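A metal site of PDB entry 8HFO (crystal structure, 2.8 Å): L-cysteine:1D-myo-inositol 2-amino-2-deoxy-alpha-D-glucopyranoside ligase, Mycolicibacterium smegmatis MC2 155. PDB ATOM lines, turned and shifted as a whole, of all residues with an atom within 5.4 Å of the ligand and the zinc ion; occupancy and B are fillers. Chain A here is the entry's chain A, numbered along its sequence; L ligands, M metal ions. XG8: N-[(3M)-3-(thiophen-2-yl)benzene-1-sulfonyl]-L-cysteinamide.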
ATOM      1  N   TYR A  42      29.463 -10.722 -30.922  1.00  0.00           N
ATOM      2  CA  TYR A  42      28.893  -9.636 -30.128  1.00  0.00           C
ATOM      3  C   TYR A  42      27.398  -9.563 -30.405  1.00  0.00           C
ATOM      4  O   TYR A  42      26.998  -9.369 -31.562  1.00  0.00           O
ATOM      5  CB  TYR A  42      29.560  -8.300 -30.423  1.00  0.00           C
ATOM      6  CG  TYR A  42      29.039  -7.136 -29.596  1.00  0.00           C
ATOM      7  CD1 TYR A  42      29.785  -6.640 -28.526  1.00  0.00           C
ATOM      8  CD2 TYR A  42      27.842  -6.500 -29.894  1.00  0.00           C
ATOM      9  CE1 TYR A  42      29.348  -5.570 -27.777  1.00  0.00           C
ATOM     10  CE2 TYR A  42      27.381  -5.429 -29.142  1.00  0.00           C
ATOM     11  CZ  TYR A  42      28.145  -4.970 -28.074  1.00  0.00           C
ATOM     12  OH  TYR A  42      27.726  -3.902 -27.317  1.00  0.00           O
ATOM     13  N   CYS A  44      23.918  -7.573 -29.266  1.00  0.00           N
ATOM     14  CA  CYS A  44      23.394  -6.405 -28.568  1.00  0.00           C
ATOM     15  C   CYS A  44      22.509  -6.848 -27.423  1.00  0.00           C
ATOM     16  O   CYS A  44      21.552  -7.614 -27.616  1.00  0.00           O
ATOM     17  CB  CYS A  44      22.617  -5.533 -29.536  1.00  0.00           C
ATOM     18  SG  CYS A  44      23.691  -4.564 -30.586  1.00  0.00           S
ATOM     19  N   GLY A  45      22.838  -6.359 -26.216  1.00  0.00           N
ATOM     20  CA  GLY A  45      22.189  -6.769 -24.995  1.00  0.00           C
ATOM     21  C   GLY A  45      20.866  -6.063 -24.752  1.00  0.00           C
ATOM     22  O   GLY A  45      20.238  -5.517 -25.654  1.00  0.00           O
ATOM     23  N   ILE A  46      20.447  -6.097 -23.511  1.00  0.00           N
ATOM     24  CA  ILE A  46      19.127  -5.598 -23.169  1.00  0.00           C
ATOM     25  C   ILE A  46      19.208  -4.139 -22.729  1.00  0.00           C
ATOM     26  O   ILE A  46      20.258  -3.641 -22.293  1.00  0.00           O
ATOM     27  CB  ILE A  46      18.459  -6.434 -22.065  1.00  0.00           C
ATOM     28  CG1 ILE A  46      19.293  -6.372 -20.788  1.00  0.00           C
ATOM     29  CG2 ILE A  46      18.294  -7.872 -22.513  1.00  0.00           C
ATOM     30  CD1 ILE A  46      18.511  -6.629 -19.531  1.00  0.00           C
ATOM     31  N   THR A  47      18.075  -3.462 -22.831  1.00  0.00           N
ATOM     32  CA  THR A  47      17.850  -2.221 -22.124  1.00  0.00           C
ATOM     33  C   THR A  47      17.042  -2.568 -20.883  1.00  0.00           C
ATOM     34  O   THR A  47      15.889  -2.995 -21.005  1.00  0.00           O
ATOM     35  CB  THR A  47      17.109  -1.222 -22.997  1.00  0.00           C
ATOM     36  OG1 THR A  47      17.822  -1.077 -24.237  1.00  0.00           O
ATOM     37  CG2 THR A  47      17.011   0.122 -22.318  1.00  0.00           C
ATOM     38  N   TYR A  49      14.650  -2.897 -18.781  1.00  0.00           N
ATOM     39  CA  TYR A  49      13.241  -2.563 -18.438  1.00  0.00           C
ATOM     40  C   TYR A  49      12.440  -3.619 -19.203  1.00  0.00           C
ATOM     41  O   TYR A  49      12.917  -3.996 -20.282  1.00  0.00           O
ATOM     42  CB  TYR A  49      12.894  -1.107 -18.743  1.00  0.00           C
ATOM     43  CG  TYR A  49      12.570  -0.758 -20.172  1.00  0.00           C
ATOM     44  CD1 TYR A  49      13.573  -0.414 -21.060  1.00  0.00           C
ATOM     45  CD2 TYR A  49      11.270  -0.731 -20.626  1.00  0.00           C
ATOM     46  CE1 TYR A  49      13.291  -0.084 -22.374  1.00  0.00           C
ATOM     47  CE2 TYR A  49      10.964  -0.400 -21.936  1.00  0.00           C
ATOM     48  CZ  TYR A  49      11.980  -0.080 -22.811  1.00  0.00           C
ATOM     49  OH  TYR A  49      11.685   0.247 -24.100  1.00  0.00           O
ATOM     50  N   HIS A  53      11.298 -10.430 -21.925  1.00  0.00           N
ATOM     51  CA  HIS A  53      10.114 -10.754 -22.746  1.00  0.00           C
ATOM     52  C   HIS A  53      10.518 -11.813 -23.766  1.00  0.00           C
ATOM     53  O   HIS A  53      11.721 -12.060 -23.919  1.00  0.00           O
ATOM     54  CB  HIS A  53       9.458  -9.510 -23.344  1.00  0.00           C
ATOM     55  CG  HIS A  53      10.334  -8.545 -24.064  1.00  0.00           C
ATOM     56  ND1 HIS A  53      10.914  -8.831 -25.281  1.00  0.00           N
ATOM     57  CD2 HIS A  53      10.661  -7.274 -23.782  1.00  0.00           C
ATOM     58  CE1 HIS A  53      11.600  -7.796 -25.693  1.00  0.00           C
ATOM     59  NE2 HIS A  53      11.459  -6.815 -24.794  1.00  0.00           N
ATOM     60  N   GLY A  55      10.653 -11.667 -26.824  1.00  0.00           N
ATOM     61  CA  GLY A  55      11.516 -11.107 -27.872  1.00  0.00           C
ATOM     62  C   GLY A  55      12.957 -11.210 -27.450  1.00  0.00           C
ATOM     63  O   GLY A  55      13.773 -11.666 -28.260  1.00  0.00           O
ATOM     64  N   HIS A  56      13.261 -10.809 -26.216  1.00  0.00           N
ATOM     65  CA  HIS A  56      14.632 -10.964 -25.692  1.00  0.00           C
ATOM     66  C   HIS A  56      14.988 -12.443 -25.750  1.00  0.00           C
ATOM     67  O   HIS A  56      16.027 -12.783 -26.299  1.00  0.00           O
ATOM     68  CB  HIS A  56      14.672 -10.588 -24.205  1.00  0.00           C
ATOM     69  CG  HIS A  56      14.565  -9.141 -23.911  1.00  0.00           C
ATOM     70  ND1 HIS A  56      13.871  -8.666 -22.821  1.00  0.00           N
ATOM     71  CD2 HIS A  56      15.069  -8.059 -24.530  1.00  0.00           C
ATOM     72  CE1 HIS A  56      13.954  -7.361 -22.787  1.00  0.00           C
ATOM     73  NE2 HIS A  56      14.671  -6.964 -23.831  1.00  0.00           N
ATOM     74  N   THR A  59      15.765 -14.047 -28.948  1.00  0.00           N
ATOM     75  CA  THR A  59      17.013 -13.529 -29.493  1.00  0.00           C
ATOM     76  C   THR A  59      18.227 -14.229 -28.882  1.00  0.00           C
ATOM     77  O   THR A  59      19.047 -14.789 -29.613  1.00  0.00           O
ATOM     78  CB  THR A  59      17.083 -11.999 -29.259  1.00  0.00           C
ATOM     79  OG1 THR A  59      16.118 -11.363 -30.093  1.00  0.00           O
ATOM     80  CG2 THR A  59      18.473 -11.466 -29.611  1.00  0.00           C
ATOM     81  N   TYR A  60      18.356 -14.216 -27.555  1.00  0.00           N
ATOM     82  CA  TYR A  60      19.562 -14.798 -26.967  1.00  0.00           C
ATOM     83  C   TYR A  60      19.562 -16.314 -27.020  1.00  0.00           C
ATOM     84  O   TYR A  60      20.640 -16.923 -26.971  1.00  0.00           O
ATOM     85  CB  TYR A  60      19.747 -14.309 -25.538  1.00  0.00           C
ATOM     86  CG  TYR A  60      19.786 -12.816 -25.547  1.00  0.00           C
ATOM     87  CD1 TYR A  60      20.915 -12.146 -25.994  1.00  0.00           C
ATOM     88  CD2 TYR A  60      18.686 -12.068 -25.131  1.00  0.00           C
ATOM     89  CE1 TYR A  60      20.956 -10.770 -26.038  1.00  0.00           C
ATOM     90  CE2 TYR A  60      18.724 -10.700 -25.170  1.00  0.00           C
ATOM     91  CZ  TYR A  60      19.851 -10.058 -25.620  1.00  0.00           C
ATOM     92  OH  TYR A  60      19.888  -8.704 -25.661  1.00  0.00           O
ATOM     93  N   ASN A  82      26.186  -6.691 -23.903  1.00  0.00           N
ATOM     94  CA  ASN A  82      26.273  -5.390 -23.198  1.00  0.00           C
ATOM     95  C   ASN A  82      24.966  -5.082 -22.502  1.00  0.00           C
ATOM     96  O   ASN A  82      24.002  -5.808 -22.718  1.00  0.00           O
ATOM     97  CB  ASN A  82      26.484  -4.241 -24.183  1.00  0.00           C
ATOM     98  CG  ASN A  82      25.374  -4.122 -25.200  1.00  0.00           C
ATOM     99  OD1 ASN A  82      25.287  -4.943 -26.118  1.00  0.00           O
ATOM    100  ND2 ASN A  82      24.527  -3.115 -25.066  1.00  0.00           N
ATOM    101  N   THR A  84      22.537  -1.695 -21.965  1.00  0.00           N
ATOM    102  CA  THR A  84      22.274  -0.278 -22.176  1.00  0.00           C
ATOM    103  C   THR A  84      21.604   0.265 -20.915  1.00  0.00           C
ATOM    104  O   THR A  84      20.394   0.542 -20.874  1.00  0.00           O
ATOM    105  CB  THR A  84      21.414  -0.071 -23.423  1.00  0.00           C
ATOM    106  OG1 THR A  84      21.809  -1.003 -24.434  1.00  0.00           O
ATOM    107  CG2 THR A  84      21.583   1.328 -23.965  1.00  0.00           C
ATOM    108  N   TRP A 228      23.808   5.989 -28.431  1.00  0.00           N
ATOM    109  CA  TRP A 228      23.490   4.568 -28.453  1.00  0.00           C
ATOM    110  C   TRP A 228      24.505   3.773 -29.277  1.00  0.00           C
ATOM    111  O   TRP A 228      25.221   2.914 -28.745  1.00  0.00           O
ATOM    112  CB  TRP A 228      22.059   4.362 -28.974  1.00  0.00           C
ATOM    113  CG  TRP A 228      21.599   2.931 -28.918  1.00  0.00           C
ATOM    114  CD1 TRP A 228      22.122   1.923 -28.150  1.00  0.00           C
ATOM    115  CD2 TRP A 228      20.520   2.340 -29.658  1.00  0.00           C
ATOM    116  NE1 TRP A 228      21.444   0.752 -28.378  1.00  0.00           N
ATOM    117  CE2 TRP A 228      20.460   0.980 -29.303  1.00  0.00           C
ATOM    118  CE3 TRP A 228      19.602   2.824 -30.603  1.00  0.00           C
ATOM    119  CZ2 TRP A 228      19.513   0.117 -29.836  1.00  0.00           C
ATOM    120  CZ3 TRP A 228      18.672   1.958 -31.127  1.00  0.00           C
ATOM    121  CH2 TRP A 228      18.632   0.624 -30.759  1.00  0.00           C
ATOM    122  N   CYS A 232      27.914   0.486 -28.458  1.00  0.00           N
ATOM    123  CA  CYS A 232      28.111  -0.903 -28.852  1.00  0.00           C
ATOM    124  C   CYS A 232      29.328  -1.084 -29.764  1.00  0.00           C
ATOM    125  O   CYS A 232      30.053  -2.076 -29.624  1.00  0.00           O
ATOM    126  CB  CYS A 232      26.846  -1.435 -29.521  1.00  0.00           C
ATOM    127  SG  CYS A 232      25.506  -1.797 -28.345  1.00  0.00           S
ATOM    128  N   GLY A 249      21.544  -9.262 -33.045  1.00  0.00           N
ATOM    129  CA  GLY A 249      20.600  -8.599 -32.175  1.00  0.00           C
ATOM    130  C   GLY A 249      19.190  -8.725 -32.717  1.00  0.00           C
ATOM    131  O   GLY A 249      18.943  -9.419 -33.712  1.00  0.00           O
ATOM    132  N   GLY A 250      18.266  -8.051 -32.042  1.00  0.00           N
ATOM    133  CA  GLY A 250      16.895  -8.011 -32.507  1.00  0.00           C
ATOM    134  C   GLY A 250      16.770  -7.376 -33.877  1.00  0.00           C
ATOM    135  O   GLY A 250      17.673  -6.708 -34.367  1.00  0.00           O
ATOM    136  N   SER A 251      15.601  -7.578 -34.494  1.00  0.00           N
ATOM    137  CA  SER A 251      15.450  -7.221 -35.906  1.00  0.00           C
ATOM    138  C   SER A 251      15.462  -5.705 -36.126  1.00  0.00           C
ATOM    139  O   SER A 251      15.928  -5.257 -37.173  1.00  0.00           O
ATOM    140  CB  SER A 251      14.159  -7.826 -36.452  1.00  0.00           C
ATOM    141  OG  SER A 251      13.116  -7.746 -35.509  1.00  0.00           O
ATOM    142  N   LEU A 253      17.376  -3.589 -35.201  1.00  0.00           N
ATOM    143  CA  LEU A 253      18.725  -3.047 -35.174  1.00  0.00           C
ATOM    144  C   LEU A 253      19.434  -3.108 -36.524  1.00  0.00           C
ATOM    145  O   LEU A 253      20.528  -2.543 -36.657  1.00  0.00           O
ATOM    146  CB  LEU A 253      19.533  -3.778 -34.095  1.00  0.00           C
ATOM    147  CG  LEU A 253      19.274  -3.411 -32.619  1.00  0.00           C
ATOM    148  CD1 LEU A 253      17.814  -3.121 -32.298  1.00  0.00           C
ATOM    149  CD2 LEU A 253      19.773  -4.538 -31.699  1.00  0.00           C
ATOM    150  N   HIS A 257      20.645   0.970 -35.779  1.00  0.00           N
ATOM    151  CA  HIS A 257      21.685   0.654 -34.811  1.00  0.00           C
ATOM    152  C   HIS A 257      22.935   0.048 -35.447  1.00  0.00           C
ATOM    153  O   HIS A 257      24.015   0.638 -35.385  1.00  0.00           O
ATOM    154  CB  HIS A 257      21.117  -0.290 -33.755  1.00  0.00           C
ATOM    155  CG  HIS A 257      21.988  -0.385 -32.547  1.00  0.00           C
ATOM    156  ND1 HIS A 257      22.686   0.707 -32.062  1.00  0.00           N
ATOM    157  CD2 HIS A 257      22.341  -1.434 -31.765  1.00  0.00           C
ATOM    158  CE1 HIS A 257      23.397   0.343 -31.010  1.00  0.00           C
ATOM    159  NE2 HIS A 257      23.213  -0.951 -30.816  1.00  0.00           N
ATOM    160  N   HIS A 258      22.798  -1.116 -36.083  1.00  0.00           N
ATOM    161  CA  HIS A 258      23.975  -1.863 -36.540  1.00  0.00           C
ATOM    162  C   HIS A 258      24.659  -1.175 -37.715  1.00  0.00           C
ATOM    163  O   HIS A 258      25.891  -1.228 -37.832  1.00  0.00           O
ATOM    164  CB  HIS A 258      23.577  -3.285 -36.899  1.00  0.00           C
ATOM    165  CG  HIS A 258      23.245  -4.140 -35.705  1.00  0.00           C
ATOM    166  ND1 HIS A 258      22.648  -5.374 -35.819  1.00  0.00           N
ATOM    167  CD2 HIS A 258      23.438  -3.929 -34.389  1.00  0.00           C
ATOM    168  CE1 HIS A 258      22.476  -5.891 -34.613  1.00  0.00           C
ATOM    169  NE2 HIS A 258      22.953  -5.026 -33.721  1.00  0.00           N
ATOM    170  N   THR A 281      17.023 -11.261 -35.504  1.00  0.00           N
ATOM    171  CA  THR A 281      16.001 -12.222 -35.121  1.00  0.00           C
ATOM    172  C   THR A 281      15.070 -11.523 -34.153  1.00  0.00           C
ATOM    173  O   THR A 281      15.458 -10.564 -33.488  1.00  0.00           O
ATOM    174  CB  THR A 281      16.620 -13.463 -34.471  1.00  0.00           C
ATOM    175  OG1 THR A 281      15.614 -14.465 -34.267  1.00  0.00           O
ATOM    176  CG2 THR A 281      17.273 -13.090 -33.134  1.00  0.00           C
ATOM    177  N   GLY A 282      13.831 -12.001 -34.069  1.00  0.00           N
ATOM    178  CA  GLY A 282      12.936 -11.403 -33.109  1.00  0.00           C
ATOM    179  C   GLY A 282      11.536 -11.956 -33.036  1.00  0.00           C
ATOM    180  O   GLY A 282      11.010 -12.523 -34.001  1.00  0.00           O
ATOM    181  N   MET A 283      10.923 -11.782 -31.872  1.00  0.00           N
ATOM    182  CA  MET A 283       9.528 -12.107 -31.637  1.00  0.00           C
ATOM    183  C   MET A 283       8.712 -10.824 -31.610  1.00  0.00           C
ATOM    184  O   MET A 283       9.239  -9.740 -31.349  1.00  0.00           O
ATOM    185  CB  MET A 283       9.365 -12.855 -30.307  1.00  0.00           C
ATOM    186  CG  MET A 283       9.085 -14.349 -30.445  1.00  0.00           C
ATOM    187  SD  MET A 283       7.334 -14.709 -30.635  1.00  0.00           S
ATOM    188  CE  MET A 283       6.657 -13.811 -29.245  1.00  0.00           C
ATOM    189  N   LYS A 290       6.360  -4.437 -31.354  1.00  0.00           N
ATOM    190  CA  LYS A 290       7.349  -4.886 -30.385  1.00  0.00           C
ATOM    191  C   LYS A 290       6.706  -5.010 -29.012  1.00  0.00           C
ATOM    192  O   LYS A 290       5.786  -4.264 -28.663  1.00  0.00           O
ATOM    193  CB  LYS A 290       8.539  -3.912 -30.355  1.00  0.00           C
ATOM    194  CG  LYS A 290       9.496  -4.087 -29.182  1.00  0.00           C
HETATM  195  N1  XG8 L   1      17.495  -3.441 -26.067  1.00  0.00           N
HETATM  196  C5  XG8 L   1      16.139  -5.659 -26.965  1.00  0.00           C
HETATM  197  C6  XG8 L   1      15.104  -6.016 -27.825  1.00  0.00           C
HETATM  198  C7  XG8 L   1      15.169  -7.221 -28.515  1.00  0.00           C
HETATM  199  C8  XG8 L   1      16.255  -8.072 -28.319  1.00  0.00           C
HETATM  200  C1  XG8 L   1      18.109  -3.030 -27.218  1.00  0.00           C
HETATM  201  C2  XG8 L   1      19.460  -2.364 -27.049  1.00  0.00           C
HETATM  202  C3  XG8 L   1      20.532  -3.080 -27.852  1.00  0.00           C
HETATM  203  C9  XG8 L   1      17.285  -7.693 -27.467  1.00  0.00           C
HETATM  204  N2  XG8 L   1      19.828  -2.228 -25.628  1.00  0.00           N
HETATM  205  O1  XG8 L   1      17.599  -3.171 -28.330  1.00  0.00           O
HETATM  206  C10 XG8 L   1      17.242  -6.486 -26.798  1.00  0.00           C
HETATM  207  C11 XG8 L   1      14.134  -7.580 -29.511  1.00  0.00           C
HETATM  208  C13 XG8 L   1      12.090  -7.696 -30.902  1.00  0.00           C
HETATM  209  C14 XG8 L   1      12.993  -8.625 -31.262  1.00  0.00           C
HETATM  210  C15 XG8 L   1      14.170  -8.568 -30.472  1.00  0.00           C
HETATM  211  O4A XG8 L   1      15.126  -3.283 -26.687  1.00  0.00           O
HETATM  212  O4B XG8 L   1      15.777  -4.533 -24.658  1.00  0.00           O
HETATM  213  S12 XG8 L   1      12.640  -6.745 -29.614  1.00  0.00           S
HETATM  214  S3  XG8 L   1      22.145  -2.246 -27.827  1.00  0.00           S
HETATM  215  S4  XG8 L   1      16.027  -4.172 -26.016  1.00  0.00           S
HETATM  216 ZN    ZN M   1      23.686  -2.637 -29.401  1.00  0.00          ZN
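C of Ile 46 touches N2 of the ligand, 3.5 Å away. Gly 55 touches the ligand. Thr 59 touches the ligand. Tyr 60 touches the ligand. Gly 250 touches the ligand (CA to C15, 3.4 Å). Leu 253 touches the ligand (CD1 to O1, 3.97 Å). Thr 281 touches the ligand. Gly 282 touches the ligand. Met 283 touches the ligand. Hydrophobic or aromatic side chains that line the ligand: His 56, Tyr 60, Trp 228 and Leu 253. Of the 25 residues printed, 18 come within 4 Å of the ligand.
The backbone NH (N) of Thr 281 sits at hydrogen-bond distance from the backbone carbonyl oxygen (O) of Gly 249 (3.2 Å). The side-chain sulfur (SG) of Cys 232 lies close to the side-chain hydroxyl (OH) of Tyr 42, 3.2 Å away. The backbone carbonyl oxygen of Cys 44 lies within hydrogen-bond range of the side-chain hydroxyl of Tyr 60 (2.8 Å). OG1 of Thr 59 sits at hydrogen-bond distance from O of Gly 55 (3.0 Å). The backbone carbonyl oxygen (O) of Leu 253 is in hydrogen-bond range of the backbone NH (N) of His 258 (2.7 Å). The backbone carbonyl oxygen (O) of Gly 45 lies close to the side-chain hydroxyl (OH) of Tyr 60, 3.2 Å away. NE2 of His 258 lies close to SG of Cys 44, 3.3 Å away. The side-chain amide oxygen of Asn 82 sits at hydrogen-bond distance from the side-chain hydroxyl of Tyr 42 (2.9 Å).
The zinc ion is bound by S3 of the ligand (2.2 Å), NE2 of His 257 (2.3 Å), SG of Cys 44 (2.3 Å) and SG of Cys 232 (2.3 Å). The zinc ion has four donor atoms within binding distance.
An oxygen (O4B) of the ligand is in hydrogen-bond range of the backbone NH of Thr 47, 3.1 Å away. OG1 of Thr 84 lies within hydrogen-bond range of N2 of the ligand (2.6 Å). OG1 of Thr 47 sits at hydrogen-bond distance from N2 of the ligand, at 2.7 Å. N2 of the ligand lies close to O of Gly 45, at 3.3 Å. ND2 of Asn 82 lies close to S3 of the ligand (3.7 Å). An oxygen (O4B) of the ligand is in hydrogen-bond range of a ring nitrogen (NE2) of His 56, at 2.8 Å. S3 of the ligand sits close to NE1 of Trp 228 (3.1 Å).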
